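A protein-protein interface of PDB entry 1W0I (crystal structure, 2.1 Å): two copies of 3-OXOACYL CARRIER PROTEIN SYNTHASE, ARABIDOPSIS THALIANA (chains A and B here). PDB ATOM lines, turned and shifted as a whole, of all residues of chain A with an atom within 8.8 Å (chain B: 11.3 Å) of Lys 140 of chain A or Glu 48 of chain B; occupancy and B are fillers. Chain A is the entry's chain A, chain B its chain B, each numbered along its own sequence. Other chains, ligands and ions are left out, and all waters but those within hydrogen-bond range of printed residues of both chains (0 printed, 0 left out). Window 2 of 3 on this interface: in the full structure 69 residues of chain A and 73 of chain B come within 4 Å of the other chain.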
ATOM      1  N   ALA A 133      22.440 -17.959  12.627  1.00  0.00           N
ATOM      2  CA  ALA A 133      22.320 -18.930  11.547  1.00  0.00           C
ATOM      3  C   ALA A 133      23.702 -19.452  11.144  1.00  0.00           C
ATOM      4  O   ALA A 133      23.876 -20.645  10.895  1.00  0.00           O
ATOM      5  CB  ALA A 133      21.619 -18.295  10.344  1.00  0.00           C
ATOM      6  N   ALA A 134      24.681 -18.554  11.085  1.00  0.00           N
ATOM      7  CA  ALA A 134      26.042 -18.935  10.724  1.00  0.00           C
ATOM      8  C   ALA A 134      26.587 -19.938  11.737  1.00  0.00           C
ATOM      9  O   ALA A 134      27.323 -20.866  11.383  1.00  0.00           O
ATOM     10  CB  ALA A 134      26.944 -17.705  10.669  1.00  0.00           C
ATOM     11  N   GLN A 135      26.227 -19.746  13.003  1.00  0.00           N
ATOM     12  CA  GLN A 135      26.673 -20.649  14.056  1.00  0.00           C
ATOM     13  C   GLN A 135      26.129 -22.055  13.793  1.00  0.00           C
ATOM     14  O   GLN A 135      26.755 -23.043  14.169  1.00  0.00           O
ATOM     15  CB  GLN A 135      26.197 -20.146  15.424  1.00  0.00           C
ATOM     16  CG  GLN A 135      26.504 -21.091  16.580  1.00  0.00           C
ATOM     17  CD  GLN A 135      25.945 -20.585  17.900  1.00  0.00           C
ATOM     18  OE1 GLN A 135      24.966 -19.834  17.925  1.00  0.00           O
ATOM     19  NE2 GLN A 135      26.557 -21.003  19.003  1.00  0.00           N
ATOM     20  N   LEU A 136      24.968 -22.140  13.144  1.00  0.00           N
ATOM     21  CA  LEU A 136      24.375 -23.435  12.834  1.00  0.00           C
ATOM     22  C   LEU A 136      25.254 -24.193  11.852  1.00  0.00           C
ATOM     23  O   LEU A 136      25.322 -25.424  11.880  1.00  0.00           O
ATOM     24  CB  LEU A 136      22.978 -23.269  12.236  1.00  0.00           C
ATOM     25  CG  LEU A 136      21.920 -22.667  13.154  1.00  0.00           C
ATOM     26  CD1 LEU A 136      20.591 -22.628  12.416  1.00  0.00           C
ATOM     27  CD2 LEU A 136      21.802 -23.497  14.431  1.00  0.00           C
ATOM     28  N   ILE A 137      25.924 -23.456  10.973  1.00  0.00           N
ATOM     29  CA  ILE A 137      26.807 -24.074   9.999  1.00  0.00           C
ATOM     30  C   ILE A 137      28.098 -24.517  10.684  1.00  0.00           C
ATOM     31  O   ILE A 137      28.565 -25.633  10.466  1.00  0.00           O
ATOM     32  CB  ILE A 137      27.153 -23.101   8.854  1.00  0.00           C
ATOM     33  CG1 ILE A 137      25.900 -22.809   8.029  1.00  0.00           C
ATOM     34  CG2 ILE A 137      28.246 -23.703   7.966  1.00  0.00           C
ATOM     35  CD1 ILE A 137      26.071 -21.672   7.036  1.00  0.00           C
ATOM     36  N   CYS A 138      28.664 -23.651  11.519  1.00  0.00           N
ATOM     37  CA  CYS A 138      29.903 -23.979  12.219  1.00  0.00           C
ATOM     38  C   CYS A 138      29.770 -25.205  13.119  1.00  0.00           C
ATOM     39  O   CYS A 138      30.713 -25.985  13.257  1.00  0.00           O
ATOM     40  CB  CYS A 138      30.368 -22.797  13.077  1.00  0.00           C
ATOM     41  SG  CYS A 138      30.762 -21.286  12.178  1.00  0.00           S
ATOM     42  N   GLU A 139      28.600 -25.374  13.729  1.00  0.00           N
ATOM     43  CA  GLU A 139      28.369 -26.494  14.640  1.00  0.00           C
ATOM     44  C   GLU A 139      27.563 -27.632  14.018  1.00  0.00           C
ATOM     45  O   GLU A 139      27.250 -28.617  14.690  1.00  0.00           O
ATOM     46  CB  GLU A 139      27.659 -25.993  15.902  1.00  0.00           C
ATOM     47  CG  GLU A 139      28.308 -24.769  16.523  1.00  0.00           C
ATOM     48  CD  GLU A 139      27.557 -24.265  17.740  1.00  0.00           C
ATOM     49  OE1 GLU A 139      26.418 -24.723  17.969  1.00  0.00           O
ATOM     50  OE2 GLU A 139      28.103 -23.408  18.464  1.00  0.00           O
ATOM     51  N   LYS A 140      27.245 -27.498  12.735  1.00  0.00           N
ATOM     52  CA  LYS A 140      26.472 -28.503  12.015  1.00  0.00           C
ATOM     53  C   LYS A 140      25.128 -28.808  12.669  1.00  0.00           C
ATOM     54  O   LYS A 140      24.838 -29.955  13.018  1.00  0.00           O
ATOM     55  CB  LYS A 140      27.271 -29.803  11.866  1.00  0.00           C
ATOM     56  CG  LYS A 140      28.431 -29.705  10.896  1.00  0.00           C
ATOM     57  CD  LYS A 140      29.701 -29.246  11.569  1.00  0.00           C
ATOM     58  CE  LYS A 140      30.479 -30.436  12.100  1.00  0.00           C
ATOM     59  NZ  LYS A 140      30.865 -31.346  10.986  1.00  0.00           N
ATOM     60  N   ARG A 141      24.315 -27.772  12.840  1.00  0.00           N
ATOM     61  CA  ARG A 141      22.990 -27.912  13.433  1.00  0.00           C
ATOM     62  C   ARG A 141      22.008 -27.112  12.581  1.00  0.00           C
ATOM     63  O   ARG A 141      21.203 -26.334  13.098  1.00  0.00           O
ATOM     64  CB  ARG A 141      22.987 -27.384  14.876  1.00  0.00           C
ATOM     65  CG  ARG A 141      23.928 -28.136  15.822  1.00  0.00           C
ATOM     66  CD  ARG A 141      23.757 -27.724  17.294  1.00  0.00           C
ATOM     67  NE  ARG A 141      24.147 -26.336  17.534  1.00  0.00           N
ATOM     68  CZ  ARG A 141      23.297 -25.321  17.668  1.00  0.00           C
ATOM     69  NH1 ARG A 141      21.988 -25.529  17.593  1.00  0.00           N
ATOM     70  NH2 ARG A 141      23.758 -24.090  17.870  1.00  0.00           N
ATOM     71  N   LEU A 142      22.081 -27.310  11.269  1.00  0.00           N
ATOM     72  CA  LEU A 142      21.220 -26.590  10.341  1.00  0.00           C
ATOM     73  C   LEU A 142      19.746 -26.931  10.469  1.00  0.00           C
ATOM     74  O   LEU A 142      18.895 -26.182   9.995  1.00  0.00           O
ATOM     75  CB  LEU A 142      21.691 -26.821   8.904  1.00  0.00           C
ATOM     76  CG  LEU A 142      22.946 -26.020   8.552  1.00  0.00           C
ATOM     77  CD1 LEU A 142      23.459 -26.421   7.186  1.00  0.00           C
ATOM     78  CD2 LEU A 142      22.614 -24.532   8.592  1.00  0.00           C
ATOM     79  N   ARG A 143      19.441 -28.052  11.112  1.00  0.00           N
ATOM     80  CA  ARG A 143      18.052 -28.453  11.290  1.00  0.00           C
ATOM     81  C   ARG A 143      17.289 -27.352  12.017  1.00  0.00           C
ATOM     82  O   ARG A 143      16.071 -27.234  11.888  1.00  0.00           O
ATOM     83  CB  ARG A 143      17.969 -29.744  12.102  1.00  0.00           C
ATOM     84  CG  ARG A 143      16.545 -30.162  12.417  1.00  0.00           C
ATOM     85  CD  ARG A 143      16.480 -31.010  13.674  1.00  0.00           C
ATOM     86  NE  ARG A 143      15.106 -31.170  14.142  1.00  0.00           N
ATOM     87  CZ  ARG A 143      14.203 -31.954  13.562  1.00  0.00           C
ATOM     88  NH1 ARG A 143      14.526 -32.664  12.487  1.00  0.00           N
ATOM     89  NH2 ARG A 143      12.974 -32.021  14.053  1.00  0.00           N
ATOM     90  N   ARG A 144      18.022 -26.545  12.774  1.00  0.00           N
ATOM     91  CA  ARG A 144      17.431 -25.450  13.534  1.00  0.00           C
ATOM     92  C   ARG A 144      17.071 -24.257  12.647  1.00  0.00           C
ATOM     93  O   ARG A 144      16.243 -23.430  13.028  1.00  0.00           O
ATOM     94  CB  ARG A 144      18.407 -24.987  14.615  1.00  0.00           C
ATOM     95  CG  ARG A 144      18.903 -26.098  15.509  1.00  0.00           C
ATOM     96  CD  ARG A 144      17.823 -26.534  16.469  1.00  0.00           C
ATOM     97  NE  ARG A 144      17.439 -25.441  17.354  1.00  0.00           N
ATOM     98  CZ  ARG A 144      16.542 -25.551  18.325  1.00  0.00           C
ATOM     99  NH1 ARG A 144      15.931 -26.710  18.536  1.00  0.00           N
ATOM    100  NH2 ARG A 144      16.260 -24.502  19.087  1.00  0.00           N
ATOM    101  N   LEU B  37      30.636 -28.375  -3.753  1.00  0.00           N
ATOM    102  CA  LEU B  37      31.124 -27.930  -2.451  1.00  0.00           C
ATOM    103  C   LEU B  37      31.817 -26.580  -2.550  1.00  0.00           C
ATOM    104  O   LEU B  37      31.686 -25.739  -1.661  1.00  0.00           O
ATOM    105  CB  LEU B  37      32.105 -28.945  -1.868  1.00  0.00           C
ATOM    106  CG  LEU B  37      31.516 -30.267  -1.395  1.00  0.00           C
ATOM    107  CD1 LEU B  37      32.629 -31.164  -0.876  1.00  0.00           C
ATOM    108  CD2 LEU B  37      30.497 -30.000  -0.303  1.00  0.00           C
ATOM    109  N   LEU B  40      29.813 -23.269  -2.223  1.00  0.00           N
ATOM    110  CA  LEU B  40      29.311 -22.851  -0.914  1.00  0.00           C
ATOM    111  C   LEU B  40      30.033 -21.611  -0.379  1.00  0.00           C
ATOM    112  O   LEU B  40      29.528 -20.927   0.511  1.00  0.00           O
ATOM    113  CB  LEU B  40      29.455 -23.996   0.092  1.00  0.00           C
ATOM    114  CG  LEU B  40      28.657 -25.275  -0.187  1.00  0.00           C
ATOM    115  CD1 LEU B  40      29.023 -26.342   0.836  1.00  0.00           C
ATOM    116  CD2 LEU B  40      27.177 -24.979  -0.138  1.00  0.00           C
ATOM    117  N   MET B  42      32.792 -21.571   1.318  1.00  0.00           N
ATOM    118  CA  MET B  42      33.192 -21.892   2.680  1.00  0.00           C
ATOM    119  C   MET B  42      34.672 -22.250   2.752  1.00  0.00           C
ATOM    120  O   MET B  42      35.051 -23.274   3.322  1.00  0.00           O
ATOM    121  CB  MET B  42      32.351 -23.057   3.200  1.00  0.00           C
ATOM    122  CG  MET B  42      30.878 -22.726   3.342  1.00  0.00           C
ATOM    123  SD  MET B  42      29.900 -24.183   3.686  1.00  0.00           S
ATOM    124  CE  MET B  42      30.440 -24.583   5.350  1.00  0.00           C
ATOM    125  N   LYS B  43      35.503 -21.395   2.169  1.00  0.00           N
ATOM    126  CA  LYS B  43      36.945 -21.604   2.151  1.00  0.00           C
ATOM    127  C   LYS B  43      37.530 -21.773   3.549  1.00  0.00           C
ATOM    128  O   LYS B  43      38.441 -22.571   3.753  1.00  0.00           O
ATOM    129  CB  LYS B  43      37.641 -20.419   1.480  1.00  0.00           C
ATOM    130  CG  LYS B  43      39.138 -20.622   1.302  1.00  0.00           C
ATOM    131  CD  LYS B  43      39.944 -19.344   1.554  1.00  0.00           C
ATOM    132  CE  LYS B  43      39.477 -18.167   0.694  1.00  0.00           C
ATOM    133  NZ  LYS B  43      38.200 -17.550   1.181  1.00  0.00           N
ATOM    134  N   SER B  44      37.001 -21.015   4.504  1.00  0.00           N
ATOM    135  CA  SER B  44      37.482 -21.042   5.875  1.00  0.00           C
ATOM    136  C   SER B  44      36.964 -22.207   6.704  1.00  0.00           C
ATOM    137  O   SER B  44      37.209 -22.267   7.909  1.00  0.00           O
ATOM    138  CB  SER B  44      37.111 -19.734   6.572  1.00  0.00           C
ATOM    139  OG  SER B  44      35.700 -19.594   6.670  1.00  0.00           O
ATOM    140  N   PHE B  45      36.236 -23.121   6.076  1.00  0.00           N
ATOM    141  CA  PHE B  45      35.704 -24.273   6.793  1.00  0.00           C
ATOM    142  C   PHE B  45      36.373 -25.568   6.340  1.00  0.00           C
ATOM    143  O   PHE B  45      36.916 -25.645   5.234  1.00  0.00           O
ATOM    144  CB  PHE B  45      34.189 -24.384   6.588  1.00  0.00           C
ATOM    145  CG  PHE B  45      33.400 -23.245   7.185  1.00  0.00           C
ATOM    146  CD1 PHE B  45      33.267 -22.037   6.506  1.00  0.00           C
ATOM    147  CD2 PHE B  45      32.776 -23.390   8.424  1.00  0.00           C
ATOM    148  CE1 PHE B  45      32.518 -20.986   7.047  1.00  0.00           C
ATOM    149  CE2 PHE B  45      32.023 -22.345   8.979  1.00  0.00           C
ATOM    150  CZ  PHE B  45      31.894 -21.142   8.287  1.00  0.00           C
ATOM    151  N   ASP B  46      36.335 -26.584   7.195  1.00  0.00           N
ATOM    152  CA  ASP B  46      36.938 -27.864   6.857  1.00  0.00           C
ATOM    153  C   ASP B  46      36.011 -28.664   5.964  1.00  0.00           C
ATOM    154  O   ASP B  46      34.838 -28.321   5.794  1.00  0.00           O
ATOM    155  CB  ASP B  46      37.277 -28.667   8.115  1.00  0.00           C
ATOM    156  CG  ASP B  46      36.072 -28.921   8.992  1.00  0.00           C
ATOM    157  OD1 ASP B  46      35.052 -29.432   8.488  1.00  0.00           O
ATOM    158  OD2 ASP B  46      36.151 -28.616  10.196  1.00  0.00           O
ATOM    159  N   GLU B  47      36.544 -29.738   5.398  1.00  0.00           N
ATOM    160  CA  GLU B  47      35.776 -30.580   4.495  1.00  0.00           C
ATOM    161  C   GLU B  47      34.532 -31.186   5.122  1.00  0.00           C
ATOM    162  O   GLU B  47      33.450 -31.139   4.536  1.00  0.00           O
ATOM    163  CB  GLU B  47      36.665 -31.693   3.937  1.00  0.00           C
ATOM    164  CG  GLU B  47      36.651 -31.749   2.425  1.00  0.00           C
ATOM    165  CD  GLU B  47      37.128 -30.447   1.793  1.00  0.00           C
ATOM    166  OE1 GLU B  47      36.786 -30.197   0.621  1.00  0.00           O
ATOM    167  OE2 GLU B  47      37.851 -29.680   2.465  1.00  0.00           O
ATOM    168  N   GLU B  48      34.689 -31.753   6.312  1.00  0.00           N
ATOM    169  CA  GLU B  48      33.577 -32.378   7.014  1.00  0.00           C
ATOM    170  C   GLU B  48      32.363 -31.446   7.141  1.00  0.00           C
ATOM    171  O   GLU B  48      31.220 -31.875   6.976  1.00  0.00           O
ATOM    172  CB  GLU B  48      34.041 -32.832   8.400  1.00  0.00           C
ATOM    173  CG  GLU B  48      33.003 -33.602   9.181  1.00  0.00           C
ATOM    174  CD  GLU B  48      33.485 -34.010  10.563  1.00  0.00           C
ATOM    175  OE1 GLU B  48      32.695 -34.649  11.293  1.00  0.00           O
ATOM    176  OE2 GLU B  48      34.644 -33.698  10.921  1.00  0.00           O
ATOM    177  N   THR B  49      32.616 -30.173   7.427  1.00  0.00           N
ATOM    178  CA  THR B  49      31.536 -29.201   7.574  1.00  0.00           C
ATOM    179  C   THR B  49      30.959 -28.802   6.212  1.00  0.00           C
ATOM    180  O   THR B  49      29.760 -28.526   6.089  1.00  0.00           O
ATOM    181  CB  THR B  49      32.025 -27.945   8.318  1.00  0.00           C
ATOM    182  OG1 THR B  49      33.114 -27.353   7.599  1.00  0.00           O
ATOM    183  CG2 THR B  49      32.501 -28.317   9.711  1.00  0.00           C
ATOM    184  N   LYS B  50      31.811 -28.771   5.191  1.00  0.00           N
ATOM    185  CA  LYS B  50      31.345 -28.444   3.849  1.00  0.00           C
ATOM    186  C   LYS B  50      30.374 -29.532   3.394  1.00  0.00           C
ATOM    187  O   LYS B  50      29.278 -29.234   2.919  1.00  0.00           O
ATOM    188  CB  LYS B  50      32.509 -28.370   2.858  1.00  0.00           C
ATOM    189  CG  LYS B  50      33.412 -27.169   3.024  1.00  0.00           C
ATOM    190  CD  LYS B  50      34.475 -27.159   1.940  1.00  0.00           C
ATOM    191  CE  LYS B  50      35.412 -25.982   2.103  1.00  0.00           C
ATOM    192  NZ  LYS B  50      36.518 -26.010   1.109  1.00  0.00           N
ATOM    193  N   LEU B  51      30.782 -30.792   3.544  1.00  0.00           N
ATOM    194  CA  LEU B  51      29.944 -31.921   3.148  1.00  0.00           C
ATOM    195  C   LEU B  51      28.619 -31.903   3.890  1.00  0.00           C
ATOM    196  O   LEU B  51      27.560 -32.100   3.295  1.00  0.00           O
ATOM    197  CB  LEU B  51      30.647 -33.248   3.435  1.00  0.00           C
ATOM    198  CG  LEU B  51      31.957 -33.520   2.703  1.00  0.00           C
ATOM    199  CD1 LEU B  51      32.630 -34.753   3.302  1.00  0.00           C
ATOM    200  CD2 LEU B  51      31.685 -33.714   1.231  1.00  0.00           C
ATOM    201  N   TYR B  52      28.683 -31.679   5.198  1.00  0.00           N
ATOM    202  CA  TYR B  52      27.479 -31.640   6.012  1.00  0.00           C
ATOM    203  C   TYR B  52      26.506 -30.604   5.469  1.00  0.00           C
ATOM    204  O   TYR B  52      25.333 -30.897   5.249  1.00  0.00           O
ATOM    205  CB  TYR B  52      27.820 -31.292   7.464  1.00  0.00           C
ATOM    206  CG  TYR B  52      26.600 -30.950   8.290  1.00  0.00           C
ATOM    207  CD1 TYR B  52      25.823 -31.948   8.882  1.00  0.00           C
ATOM    208  CD2 TYR B  52      26.181 -29.625   8.418  1.00  0.00           C
ATOM    209  CE1 TYR B  52      24.652 -31.629   9.576  1.00  0.00           C
ATOM    210  CE2 TYR B  52      25.018 -29.297   9.102  1.00  0.00           C
ATOM    211  CZ  TYR B  52      24.257 -30.298   9.679  1.00  0.00           C
ATOM    212  OH  TYR B  52      23.096 -29.963  10.340  1.00  0.00           O
ATOM    213  N   THR B  53      27.013 -29.391   5.264  1.00  0.00           N
ATOM    214  CA  THR B  53      26.211 -28.276   4.771  1.00  0.00           C
ATOM    215  C   THR B  53      25.613 -28.585   3.400  1.00  0.00           C
ATOM    216  O   THR B  53      24.408 -28.443   3.190  1.00  0.00           O
ATOM    217  CB  THR B  53      27.067 -26.989   4.690  1.00  0.00           C
ATOM    218  OG1 THR B  53      27.711 -26.776   5.954  1.00  0.00           O
ATOM    219  CG2 THR B  53      26.197 -25.777   4.364  1.00  0.00           C
ATOM    220  N   PHE B  54      26.459 -29.012   2.473  1.00  0.00           N
ATOM    221  CA  PHE B  54      26.008 -29.341   1.129  1.00  0.00           C
ATOM    222  C   PHE B  54      24.885 -30.375   1.181  1.00  0.00           C
ATOM    223  O   PHE B  54      23.895 -30.266   0.460  1.00  0.00           O
ATOM    224  CB  PHE B  54      27.175 -29.888   0.307  1.00  0.00           C
ATOM    225  CG  PHE B  54      26.846 -30.106  -1.141  1.00  0.00           C
ATOM    226  CD1 PHE B  54      26.754 -29.028  -2.016  1.00  0.00           C
ATOM    227  CD2 PHE B  54      26.602 -31.387  -1.628  1.00  0.00           C
ATOM    228  CE1 PHE B  54      26.424 -29.222  -3.356  1.00  0.00           C
ATOM    229  CE2 PHE B  54      26.270 -31.593  -2.966  1.00  0.00           C
ATOM    230  CZ  PHE B  54      26.182 -30.509  -3.832  1.00  0.00           C
ATOM    231  N   ASP B  55      25.040 -31.373   2.044  1.00  0.00           N
ATOM    232  CA  ASP B  55      24.046 -32.432   2.180  1.00  0.00           C
ATOM    233  C   ASP B  55      22.696 -31.935   2.685  1.00  0.00           C
ATOM    234  O   ASP B  55      21.662 -32.542   2.403  1.00  0.00           O
ATOM    235  CB  ASP B  55      24.559 -33.521   3.123  1.00  0.00           C
ATOM    236  CG  ASP B  55      23.637 -34.725   3.175  1.00  0.00           C
ATOM    237  OD1 ASP B  55      23.578 -35.471   2.174  1.00  0.00           O
ATOM    238  OD2 ASP B  55      22.963 -34.922   4.211  1.00  0.00           O
ATOM    239  N   GLN B  56      22.705 -30.837   3.435  1.00  0.00           N
ATOM    240  CA  GLN B  56      21.474 -30.273   3.986  1.00  0.00           C
ATOM    241  C   GLN B  56      20.712 -29.424   2.974  1.00  0.00           C
ATOM    242  O   GLN B  56      19.532 -29.143   3.163  1.00  0.00           O
ATOM    243  CB  GLN B  56      21.791 -29.411   5.212  1.00  0.00           C
ATOM    244  CG  GLN B  56      22.573 -30.117   6.308  1.00  0.00           C
ATOM    245  CD  GLN B  56      21.864 -31.350   6.831  1.00  0.00           C
ATOM    246  OE1 GLN B  56      20.687 -31.298   7.186  1.00  0.00           O
ATOM    247  NE2 GLN B  56      22.585 -32.466   6.893  1.00  0.00           N
ATOM    248  N   VAL B 131      29.100 -14.644   7.467  1.00  0.00           N
ATOM    249  CA  VAL B 131      29.248 -16.016   7.938  1.00  0.00           C
ATOM    250  C   VAL B 131      30.697 -16.256   8.373  1.00  0.00           C
ATOM    251  O   VAL B 131      30.948 -16.884   9.401  1.00  0.00           O
ATOM    252  CB  VAL B 131      28.871 -17.042   6.824  1.00  0.00           C
ATOM    253  CG1 VAL B 131      29.304 -18.447   7.225  1.00  0.00           C
ATOM    254  CG2 VAL B 131      27.358 -17.024   6.581  1.00  0.00           C
ATOM    255  N   GLN B 135      32.154 -17.046  12.093  1.00  0.00           N
ATOM    256  CA  GLN B 135      32.999 -18.188  12.417  1.00  0.00           C
ATOM    257  C   GLN B 135      34.158 -17.762  13.330  1.00  0.00           C
ATOM    258  O   GLN B 135      34.631 -18.557  14.140  1.00  0.00           O
ATOM    259  CB  GLN B 135      33.545 -18.832  11.133  1.00  0.00           C
ATOM    260  CG  GLN B 135      34.577 -19.931  11.386  1.00  0.00           C
ATOM    261  CD  GLN B 135      35.173 -20.503  10.107  1.00  0.00           C
ATOM    262  OE1 GLN B 135      35.644 -19.765   9.244  1.00  0.00           O
ATOM    263  NE2 GLN B 135      35.171 -21.827   9.995  1.00  0.00           N
ATOM    264  N   CYS B 138      32.798 -18.029  16.787  1.00  0.00           N
ATOM    265  CA  CYS B 138      32.697 -19.422  17.221  1.00  0.00           C
ATOM    266  C   CYS B 138      34.062 -20.030  17.511  1.00  0.00           C
ATOM    267  O   CYS B 138      34.189 -20.933  18.338  1.00  0.00           O
ATOM    268  CB  CYS B 138      32.013 -20.274  16.152  1.00  0.00           C
ATOM    269  SG  CYS B 138      30.331 -19.782  15.754  1.00  0.00           S
ATOM    270  N   GLU B 139      35.084 -19.537  16.823  1.00  0.00           N
ATOM    271  CA  GLU B 139      36.433 -20.058  17.000  1.00  0.00           C
ATOM    272  C   GLU B 139      37.341 -19.126  17.787  1.00  0.00           C
ATOM    273  O   GLU B 139      38.543 -19.366  17.897  1.00  0.00           O
ATOM    274  CB  GLU B 139      37.050 -20.351  15.633  1.00  0.00           C
ATOM    275  CG  GLU B 139      36.527 -21.630  15.008  1.00  0.00           C
ATOM    276  CD  GLU B 139      36.961 -21.787  13.567  1.00  0.00           C
ATOM    277  OE1 GLU B 139      38.111 -21.417  13.244  1.00  0.00           O
ATOM    278  OE2 GLU B 139      36.156 -22.294  12.759  1.00  0.00           O
ATOM    279  N   ALA B 212      26.576 -20.922   0.934  1.00  0.00           N
ATOM    280  CA  ALA B 212      25.982 -21.825   1.902  1.00  0.00           C
ATOM    281  C   ALA B 212      24.703 -21.331   2.567  1.00  0.00           C
ATOM    282  O   ALA B 212      23.638 -21.917   2.386  1.00  0.00           O
ATOM    283  CB  ALA B 212      27.014 -22.169   2.964  1.00  0.00           C
ATOM    284  N   LEU B 213      24.814 -20.250   3.334  1.00  0.00           N
ATOM    285  CA  LEU B 213      23.669 -19.713   4.060  1.00  0.00           C
ATOM    286  C   LEU B 213      22.560 -19.147   3.179  1.00  0.00           C
ATOM    287  O   LEU B 213      21.380 -19.257   3.519  1.00  0.00           O
ATOM    288  CB  LEU B 213      24.137 -18.654   5.063  1.00  0.00           C
ATOM    289  CG  LEU B 213      23.110 -18.117   6.060  1.00  0.00           C
ATOM    290  CD1 LEU B 213      22.430 -19.274   6.791  1.00  0.00           C
ATOM    291  CD2 LEU B 213      23.811 -17.201   7.054  1.00  0.00           C
ATOM    292  N   ALA B 216      20.868 -22.258   1.859  1.00  0.00           N
ATOM    293  CA  ALA B 216      20.181 -22.935   2.960  1.00  0.00           C
ATOM    294  C   ALA B 216      18.966 -22.124   3.416  1.00  0.00           C
ATOM    295  O   ALA B 216      17.909 -22.684   3.708  1.00  0.00           O
ATOM    296  CB  ALA B 216      21.139 -23.147   4.133  1.00  0.00           C
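The side-chain amino group of Lys 140 of chain A is in salt-bridge range of the side-chain carboxylate of Glu 48 of chain B.
The backbone carbonyl oxygen of Lys 140 of chain A sits at hydrogen-bond distance from the side-chain hydroxyl of Tyr 52 of chain B.
N of Leu 142 of chain A sits at hydrogen-bond distance from OH of Tyr 52 of chain B (3.0 Å).
N of Arg 141 of chain A is in hydrogen-bond range of O of Leu 136 of chain A (2.7 Å).
OE1 of Glu 139 of chain A is in salt-bridge range of NH2 of Arg 141 of chain A, 2.7 Å away.
OG of Ser 44 of chain B lies within hydrogen-bond range of OE1 of Gln 135 of chain B (2.6 Å).
OD1 of Asp 46 of chain B sits at hydrogen-bond distance from N of Glu 48 of chain B (3.2 Å).
The backbone carbonyl oxygen (O) of Asp 46 of chain B sits at hydrogen-bond distance from the side-chain hydroxyl (OG1) of Thr 49 of chain B (2.7 Å).
The side-chain carboxylate (OE2) of Glu 139 of chain B is in hydrogen-bond range of the side-chain amide nitrogen (NE2) of Gln 135 of chain B (3.0 Å).
Among the printed residues, merely in contact across the chains: Lys 140 of chain A with Thr 49 of chain B (3.5 Å), Ile 137 of chain A with Met 42 of chain B (3.5 Å), Arg 141 of chain A with Tyr 52 of chain B (3.5 Å), Cys 138 of chain A with Phe 45 of chain B (3.6 Å), Ile 137 of chain A with Thr 53 of chain B (3.7 Å), Ala 133 of chain A with Leu 213 of chain B (3.8 Å), Cys 138 of chain A with Gln 135 of chain B (3.8 Å), Leu 142 of chain A with Gln 56 of chain B (3.9 Å), Cys 138 of chain A with Cys 138 of chain B (3.9 Å), Ala 134 of chain A with Val 131 of chain B (3.95 Å) and Leu 142 of chain A with Thr 53 of chain B (3.98 Å).
Of the printed residues of chain B, Lys 140 of chain A touches Glu 48, Thr 49 and Tyr 52.
Of the printed residues of chain A, Glu 48 of chain B touches Lys 140 (3.6 Å).
Cys 138 of chain A touches three residues of chain B.
No residue of chain B comes within 4 Å of Glu 139 of chain A.
Printed residues of chain A within 4 Å of Met 42 of chain B: Ile 137.
Of the printed residues of chain B, Ala 134 of chain A touches Val 131.
Of the printed residues of chain A, Cys 138 of chain B touches Cys 138 (3.9 Å).
Printed residues of chain A within 4 Å of Tyr 52 of chain B: Lys 140, Arg 141 and Leu 142.
Arg 144 of chain A touches none of the printed residues of chain B.
Leu 136 of chain A touches none of the printed residues of chain B.
The nearest residue of chain A that does not touch Glu 48 of chain B is Ile 137 of chain A (7.6 Å).
Hydrophobic or aromatic side chains of chain B that line the printed part of chain A: Met 42, Phe 45, Tyr 52 and Leu 213.
Among the printed residues, Asp or Glu carboxylates within 4 Å of a Lys or Arg side-chain nitrogen of the other chain: Lys 140 of chain A with Glu 48 of chain B (3.8 Å).
Cys 138 of chain A touches Gln 135 of chain B, but with the chains exchanged Gln 135 of chain A does not touch Cys 138 of chain B (4.1 Å).
Cys 138 of chain B touches its own counterpart, Cys 138 of chain A.
Positions printed for both chains: 135, 138 and 139.
Of the 14 pairs that touch across the chains among the printed residues, 1 has its exchanged pair printed and touching as well.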
